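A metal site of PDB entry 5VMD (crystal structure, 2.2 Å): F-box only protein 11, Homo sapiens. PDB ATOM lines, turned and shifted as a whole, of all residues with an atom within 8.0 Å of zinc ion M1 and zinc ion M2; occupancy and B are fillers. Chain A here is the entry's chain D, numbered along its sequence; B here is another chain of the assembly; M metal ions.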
ATOM      1  N   ALA A  36      -4.443 -28.357  -9.656  1.00  0.00           N
ATOM      2  CA  ALA A  36      -4.197 -27.278 -10.596  1.00  0.00           C
ATOM      3  C   ALA A  36      -2.699 -27.054 -10.676  1.00  0.00           C
ATOM      4  O   ALA A  36      -2.040 -26.886  -9.644  1.00  0.00           O
ATOM      5  CB  ALA A  36      -4.904 -25.984 -10.167  1.00  0.00           C
ATOM      6  N   ILE A  37      -2.163 -27.060 -11.890  1.00  0.00           N
ATOM      7  CA  ILE A  37      -0.720 -27.079 -12.089  1.00  0.00           C
ATOM      8  C   ILE A  37      -0.346 -26.025 -13.127  1.00  0.00           C
ATOM      9  O   ILE A  37      -1.032 -25.882 -14.145  1.00  0.00           O
ATOM     10  CB  ILE A  37      -0.230 -28.469 -12.523  1.00  0.00           C
ATOM     11  CG1 ILE A  37      -0.627 -29.497 -11.462  1.00  0.00           C
ATOM     12  CG2 ILE A  37       1.269 -28.448 -12.757  1.00  0.00           C
ATOM     13  CD1 ILE A  37      -0.492 -30.918 -11.916  1.00  0.00           C
ATOM     14  N   CYS A  38       0.733 -25.300 -12.862  1.00  0.00           N
ATOM     15  CA  CYS A  38       1.194 -24.279 -13.788  1.00  0.00           C
ATOM     16  C   CYS A  38       1.872 -24.923 -14.996  1.00  0.00           C
ATOM     17  O   CYS A  38       2.257 -26.099 -14.967  1.00  0.00           O
ATOM     18  CB  CYS A  38       2.143 -23.315 -13.079  1.00  0.00           C
ATOM     19  SG  CYS A  38       3.748 -24.042 -12.719  1.00  0.00           S
ATOM     20  N   VAL A  39       2.026 -24.134 -16.059  1.00  0.00           N
ATOM     21  CA  VAL A  39       2.543 -24.694 -17.308  1.00  0.00           C
ATOM     22  C   VAL A  39       3.986 -25.166 -17.132  1.00  0.00           C
ATOM     23  O   VAL A  39       4.372 -26.221 -17.652  1.00  0.00           O
ATOM     24  CB  VAL A  39       2.411 -23.672 -18.449  1.00  0.00           C
ATOM     25  CG1 VAL A  39       3.257 -22.442 -18.166  1.00  0.00           C
ATOM     26  CG2 VAL A  39       2.819 -24.302 -19.779  1.00  0.00           C
ATOM     27  N   ASN A  40       4.801 -24.395 -16.407  1.00  0.00           N
ATOM     28  CA  ASN A  40       6.189 -24.794 -16.206  1.00  0.00           C
ATOM     29  C   ASN A  40       6.279 -26.137 -15.497  1.00  0.00           C
ATOM     30  O   ASN A  40       7.094 -26.992 -15.857  1.00  0.00           O
ATOM     31  CB  ASN A  40       6.952 -23.722 -15.422  1.00  0.00           C
ATOM     32  CG  ASN A  40       7.238 -22.486 -16.246  1.00  0.00           C
ATOM     33  OD1 ASN A  40       7.097 -22.483 -17.462  1.00  0.00           O
ATOM     34  ND2 ASN A  40       7.682 -21.420 -15.571  1.00  0.00           N
ATOM     35  N   CYS A  41       5.447 -26.337 -14.471  1.00  0.00           N
ATOM     36  CA  CYS A  41       5.476 -27.602 -13.742  1.00  0.00           C
ATOM     37  C   CYS A  41       4.947 -28.745 -14.600  1.00  0.00           C
ATOM     38  O   CYS A  41       5.470 -29.858 -14.550  1.00  0.00           O
ATOM     39  CB  CYS A  41       4.688 -27.475 -12.446  1.00  0.00           C
ATOM     40  SG  CYS A  41       5.613 -26.578 -11.158  1.00  0.00           S
ATOM     41  N   ILE A  42       3.910 -28.481 -15.405  1.00  0.00           N
ATOM     42  CA  ILE A  42       3.318 -29.542 -16.207  1.00  0.00           C
ATOM     43  C   ILE A  42       4.317 -30.063 -17.250  1.00  0.00           C
ATOM     44  O   ILE A  42       4.366 -31.264 -17.527  1.00  0.00           O
ATOM     45  CB  ILE A  42       2.007 -29.056 -16.851  1.00  0.00           C
ATOM     46  CG1 ILE A  42       1.049 -30.223 -17.067  1.00  0.00           C
ATOM     47  CG2 ILE A  42       2.283 -28.333 -18.160  1.00  0.00           C
ATOM     48  CD1 ILE A  42       0.531 -30.835 -15.784  1.00  0.00           C
ATOM     49  N   LYS A  43       5.117 -29.168 -17.819  1.00  0.00           N
ATOM     50  CA  LYS A  43       6.086 -29.601 -18.832  1.00  0.00           C
ATOM     51  C   LYS A  43       7.322 -30.239 -18.207  1.00  0.00           C
ATOM     52  O   LYS A  43       7.895 -31.175 -18.783  1.00  0.00           O
ATOM     53  CB  LYS A  43       6.484 -28.426 -19.725  1.00  0.00           C
ATOM     54  CG  LYS A  43       5.370 -27.911 -20.624  1.00  0.00           C
ATOM     55  CD  LYS A  43       5.925 -26.955 -21.680  1.00  0.00           C
ATOM     56  CE  LYS A  43       4.965 -26.782 -22.847  1.00  0.00           C
ATOM     57  NZ  LYS A  43       3.835 -25.874 -22.541  1.00  0.00           N
ATOM     58  N   LYS A  44       7.754 -29.759 -17.048  1.00  0.00           N
ATOM     59  CA  LYS A  44       8.997 -30.221 -16.433  1.00  0.00           C
ATOM     60  C   LYS A  44       8.781 -31.225 -15.312  1.00  0.00           C
ATOM     61  O   LYS A  44       9.488 -32.237 -15.254  1.00  0.00           O
ATOM     62  CB  LYS A  44       9.802 -29.023 -15.910  1.00  0.00           C
ATOM     63  CG  LYS A  44      11.230 -29.370 -15.521  1.00  0.00           C
ATOM     64  CD  LYS A  44      12.099 -28.129 -15.432  1.00  0.00           C
ATOM     65  CE  LYS A  44      13.549 -28.490 -15.088  1.00  0.00           C
ATOM     66  NZ  LYS A  44      14.414 -27.285 -14.977  1.00  0.00           N
ATOM     67  N   CYS A  45       7.816 -30.996 -14.425  1.00  0.00           N
ATOM     68  CA  CYS A  45       7.558 -31.903 -13.316  1.00  0.00           C
ATOM     69  C   CYS A  45       6.589 -33.018 -13.680  1.00  0.00           C
ATOM     70  O   CYS A  45       6.459 -33.977 -12.903  1.00  0.00           O
ATOM     71  CB  CYS A  45       7.009 -31.131 -12.108  1.00  0.00           C
ATOM     72  SG  CYS A  45       8.023 -29.746 -11.595  1.00  0.00           S
ATOM     73  N   HIS A  46       5.912 -32.925 -14.819  1.00  0.00           N
ATOM     74  CA  HIS A  46       4.901 -33.901 -15.195  1.00  0.00           C
ATOM     75  C   HIS A  46       5.044 -34.324 -16.655  1.00  0.00           C
ATOM     76  O   HIS A  46       4.058 -34.650 -17.325  1.00  0.00           O
ATOM     77  CB  HIS A  46       3.497 -33.332 -14.920  1.00  0.00           C
ATOM     78  CG  HIS A  46       3.323 -32.815 -13.528  1.00  0.00           C
ATOM     79  ND1 HIS A  46       2.789 -33.569 -12.505  1.00  0.00           N
ATOM     80  CD2 HIS A  46       3.655 -31.621 -12.964  1.00  0.00           C
ATOM     81  CE1 HIS A  46       2.778 -32.864 -11.388  1.00  0.00           C
ATOM     82  NE2 HIS A  46       3.301 -31.685 -11.640  1.00  0.00           N
ATOM     83  N   PHE B  59      -3.035 -18.293  -9.808  1.00  0.00           N
ATOM     84  CA  PHE B  59      -1.619 -18.628  -9.781  1.00  0.00           C
ATOM     85  C   PHE B  59      -1.280 -19.783  -8.859  1.00  0.00           C
ATOM     86  O   PHE B  59      -0.101 -20.153  -8.742  1.00  0.00           O
ATOM     87  CB  PHE B  59      -0.798 -17.391  -9.410  1.00  0.00           C
ATOM     88  CG  PHE B  59      -0.964 -16.259 -10.379  1.00  0.00           C
ATOM     89  CD1 PHE B  59      -0.583 -16.407 -11.703  1.00  0.00           C
ATOM     90  CD2 PHE B  59      -1.511 -15.042  -9.979  1.00  0.00           C
ATOM     91  CE1 PHE B  59      -0.748 -15.381 -12.614  1.00  0.00           C
ATOM     92  CE2 PHE B  59      -1.670 -14.009 -10.891  1.00  0.00           C
ATOM     93  CZ  PHE B  59      -1.286 -14.175 -12.216  1.00  0.00           C
ATOM     94  N   PHE B  60      -2.268 -20.394  -8.202  1.00  0.00           N
ATOM     95  CA  PHE B  60      -1.962 -21.508  -7.327  1.00  0.00           C
ATOM     96  C   PHE B  60      -1.545 -22.726  -8.132  1.00  0.00           C
ATOM     97  O   PHE B  60      -2.137 -23.047  -9.169  1.00  0.00           O
ATOM     98  CB  PHE B  60      -3.156 -21.844  -6.439  1.00  0.00           C
ATOM     99  CG  PHE B  60      -2.913 -23.033  -5.534  1.00  0.00           C
ATOM    100  CD1 PHE B  60      -2.196 -22.879  -4.366  1.00  0.00           C
ATOM    101  CD2 PHE B  60      -3.381 -24.293  -5.878  1.00  0.00           C
ATOM    102  CE1 PHE B  60      -1.950 -23.968  -3.541  1.00  0.00           C
ATOM    103  CE2 PHE B  60      -3.140 -25.376  -5.059  1.00  0.00           C
ATOM    104  CZ  PHE B  60      -2.420 -25.210  -3.885  1.00  0.00           C
ATOM    105  N   CYS B  61      -0.541 -23.444  -7.624  1.00  0.00           N
ATOM    106  CA  CYS B  61      -0.043 -24.655  -8.282  1.00  0.00           C
ATOM    107  C   CYS B  61       0.179 -25.720  -7.220  1.00  0.00           C
ATOM    108  O   CYS B  61       0.983 -25.526  -6.310  1.00  0.00           O
ATOM    109  CB  CYS B  61       1.259 -24.383  -9.038  1.00  0.00           C
ATOM    110  SG  CYS B  61       2.024 -25.870  -9.784  1.00  0.00           S
ATOM    111  N   ASP B  62      -0.558 -26.827  -7.338  1.00  0.00           N
ATOM    112  CA  ASP B  62      -0.408 -27.915  -6.368  1.00  0.00           C
ATOM    113  C   ASP B  62       1.004 -28.473  -6.352  1.00  0.00           C
ATOM    114  O   ASP B  62       1.495 -28.901  -5.304  1.00  0.00           O
ATOM    115  CB  ASP B  62      -1.391 -29.039  -6.681  1.00  0.00           C
ATOM    116  CG  ASP B  62      -2.789 -28.723  -6.205  1.00  0.00           C
ATOM    117  OD1 ASP B  62      -2.998 -28.684  -4.961  1.00  0.00           O
ATOM    118  OD2 ASP B  62      -3.681 -28.539  -7.060  1.00  0.00           O
ATOM    119  N   CYS B  63       1.679 -28.457  -7.503  1.00  0.00           N
ATOM    120  CA  CYS B  63       3.021 -29.014  -7.594  1.00  0.00           C
ATOM    121  C   CYS B  63       4.008 -28.203  -6.759  1.00  0.00           C
ATOM    122  O   CYS B  63       4.691 -28.744  -5.885  1.00  0.00           O
ATOM    123  CB  CYS B  63       3.457 -29.077  -9.053  1.00  0.00           C
ATOM    124  SG  CYS B  63       4.965 -30.020  -9.334  1.00  0.00           S
ATOM    125  N   GLY B  64       4.108 -26.902  -7.039  1.00  0.00           N
ATOM    126  CA  GLY B  64       4.980 -26.052  -6.242  1.00  0.00           C
ATOM    127  C   GLY B  64       4.548 -25.924  -4.798  1.00  0.00           C
ATOM    128  O   GLY B  64       5.376 -25.714  -3.912  1.00  0.00           O
ATOM    129  N   ALA B  65       3.250 -26.057  -4.534  1.00  0.00           N
ATOM    130  CA  ALA B  65       2.763 -25.968  -3.163  1.00  0.00           C
ATOM    131  C   ALA B  65       3.097 -27.199  -2.338  1.00  0.00           C
ATOM    132  O   ALA B  65       2.960 -27.149  -1.102  1.00  0.00           O
ATOM    133  CB  ALA B  65       1.235 -25.746  -3.163  1.00  0.00           C
ATOM    134  N   GLY B  66       3.551 -28.278  -2.964  1.00  0.00           N
ATOM    135  CA  GLY B  66       3.910 -29.475  -2.228  1.00  0.00           C
ATOM    136  C   GLY B  66       2.749 -30.353  -1.821  1.00  0.00           C
ATOM    137  O   GLY B  66       2.872 -31.118  -0.859  1.00  0.00           O
ATOM    138  N   LEU B  68       1.268 -32.615  -3.912  1.00  0.00           N
ATOM    139  CA  LEU B  68       1.238 -33.826  -4.721  1.00  0.00           C
ATOM    140  C   LEU B  68       2.198 -34.880  -4.183  1.00  0.00           C
ATOM    141  O   LEU B  68       3.095 -34.594  -3.391  1.00  0.00           O
ATOM    142  CB  LEU B  68       1.600 -33.503  -6.176  1.00  0.00           C
ATOM    143  CG  LEU B  68       0.789 -32.383  -6.822  1.00  0.00           C
ATOM    144  CD1 LEU B  68       1.244 -32.167  -8.272  1.00  0.00           C
ATOM    145  CD2 LEU B  68      -0.698 -32.675  -6.743  1.00  0.00           C
ATOM    146  N   ASN B  70       4.652 -36.406  -5.510  1.00  0.00           N
ATOM    147  CA  ASN B  70       6.057 -36.150  -5.757  1.00  0.00           C
ATOM    148  C   ASN B  70       6.394 -34.695  -5.473  1.00  0.00           C
ATOM    149  O   ASN B  70       5.578 -33.812  -5.746  1.00  0.00           O
ATOM    150  CB  ASN B  70       6.415 -36.448  -7.220  1.00  0.00           C
ATOM    151  CG  ASN B  70       6.099 -37.851  -7.621  1.00  0.00           C
ATOM    152  OD1 ASN B  70       6.321 -38.808  -6.859  1.00  0.00           O
ATOM    153  ND2 ASN B  70       5.543 -38.013  -8.813  1.00  0.00           N
ATOM    154  N   PRO B  71       7.578 -34.400  -4.938  1.00  0.00           N
ATOM    155  CA  PRO B  71       7.945 -32.998  -4.735  1.00  0.00           C
ATOM    156  C   PRO B  71       8.191 -32.303  -6.054  1.00  0.00           C
ATOM    157  O   PRO B  71       8.576 -32.916  -7.062  1.00  0.00           O
ATOM    158  CB  PRO B  71       9.230 -33.080  -3.886  1.00  0.00           C
ATOM    159  CG  PRO B  71       9.220 -34.479  -3.316  1.00  0.00           C
ATOM    160  CD  PRO B  71       8.547 -35.329  -4.346  1.00  0.00           C
ATOM    161  N   CYS B  72       7.948 -30.998  -6.064  1.00  0.00           N
ATOM    162  CA  CYS B  72       8.168 -30.220  -7.268  1.00  0.00           C
ATOM    163  C   CYS B  72       9.642 -30.232  -7.641  1.00  0.00           C
ATOM    164  O   CYS B  72      10.517 -30.143  -6.780  1.00  0.00           O
ATOM    165  CB  CYS B  72       7.671 -28.789  -7.040  1.00  0.00           C
ATOM    166  SG  CYS B  72       8.028 -27.636  -8.354  1.00  0.00           S
ATOM    167  N   THR B  73       9.933 -30.344  -8.936  1.00  0.00           N
ATOM    168  CA  THR B  73      11.310 -30.342  -9.413  1.00  0.00           C
ATOM    169  C   THR B  73      11.839 -28.945  -9.688  1.00  0.00           C
ATOM    170  O   THR B  73      12.954 -28.812 -10.189  1.00  0.00           O
ATOM    171  CB  THR B  73      11.460 -31.204 -10.677  1.00  0.00           C
ATOM    172  OG1 THR B  73      10.896 -30.512 -11.799  1.00  0.00           O
ATOM    173  CG2 THR B  73      10.755 -32.536 -10.505  1.00  0.00           C
ATOM    174  N   LEU B  74      11.063 -27.907  -9.377  1.00  0.00           N
ATOM    175  CA  LEU B  74      11.462 -26.538  -9.667  1.00  0.00           C
ATOM    176  C   LEU B  74      11.637 -25.703  -8.400  1.00  0.00           C
ATOM    177  O   LEU B  74      12.382 -26.076  -7.500  1.00  0.00           O
ATOM    178  CB  LEU B  74      10.439 -25.861 -10.585  1.00  0.00           C
ATOM    179  CG  LEU B  74      10.204 -26.559 -11.925  1.00  0.00           C
ATOM    180  CD1 LEU B  74       9.144 -25.819 -12.733  1.00  0.00           C
ATOM    181  CD2 LEU B  74      11.510 -26.661 -12.692  1.00  0.00           C
HETATM  182 ZN    ZN M   1       4.081 -24.956 -10.483  1.00  0.00          ZN
HETATM  183 ZN    ZN M   2       6.540 -28.543 -10.060  1.00  0.00          ZN
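N of Cys 63 of chain B lies close to SG of Cys 61 of chain B, at 3.5 Å. The side-chain sulfur (SG) of Cys 72 of chain B sits close to the backbone NH (N) of Leu 74 of chain B. SG of Cys 61 of chain B lies close to N of Gly 64 of chain B (3.6 Å). The side-chain hydroxyl (OG1) of Thr 73 of chain B lies close to the side-chain sulfur (SG) of Cys 45, 3.0 Å away. SG of Cys 63 of chain B sits close to NE2 of His 46, 3.3 Å away. O of Cys 41 sits close to N of His 46 (3.1 Å).
N of Gly 64 of chain B touches zinc ion M1, at 3.96 Å. Of the 25 residues printed, 4 come within 4 Å of zinc ion M1. The nearest printed residue that does not touch zinc ion M1 is Cys 63 of chain B (4.4 Å).
Within 4 Å of zinc ion M2: Cys 41, Cys 45, Cys 63 of chain B and Cys 72 of chain B.
Zinc ion M1 is bound by the side-chain sulfur (SG) of Cys 41 (2.3 Å). The side-chain sulfur (SG) of Cys 61 of chain B binds zinc ion M1 (2.4 Å). Zinc ion M1 is bound by SG of Cys 38 (2.4 Å).
Zinc ion M2 is bound by SG of Cys 63 of chain B (2.3 Å), SG of Cys 41 (2.4 Å), SG of Cys 72 of chain B (2.4 Å) and SG of Cys 45 (2.5 Å).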
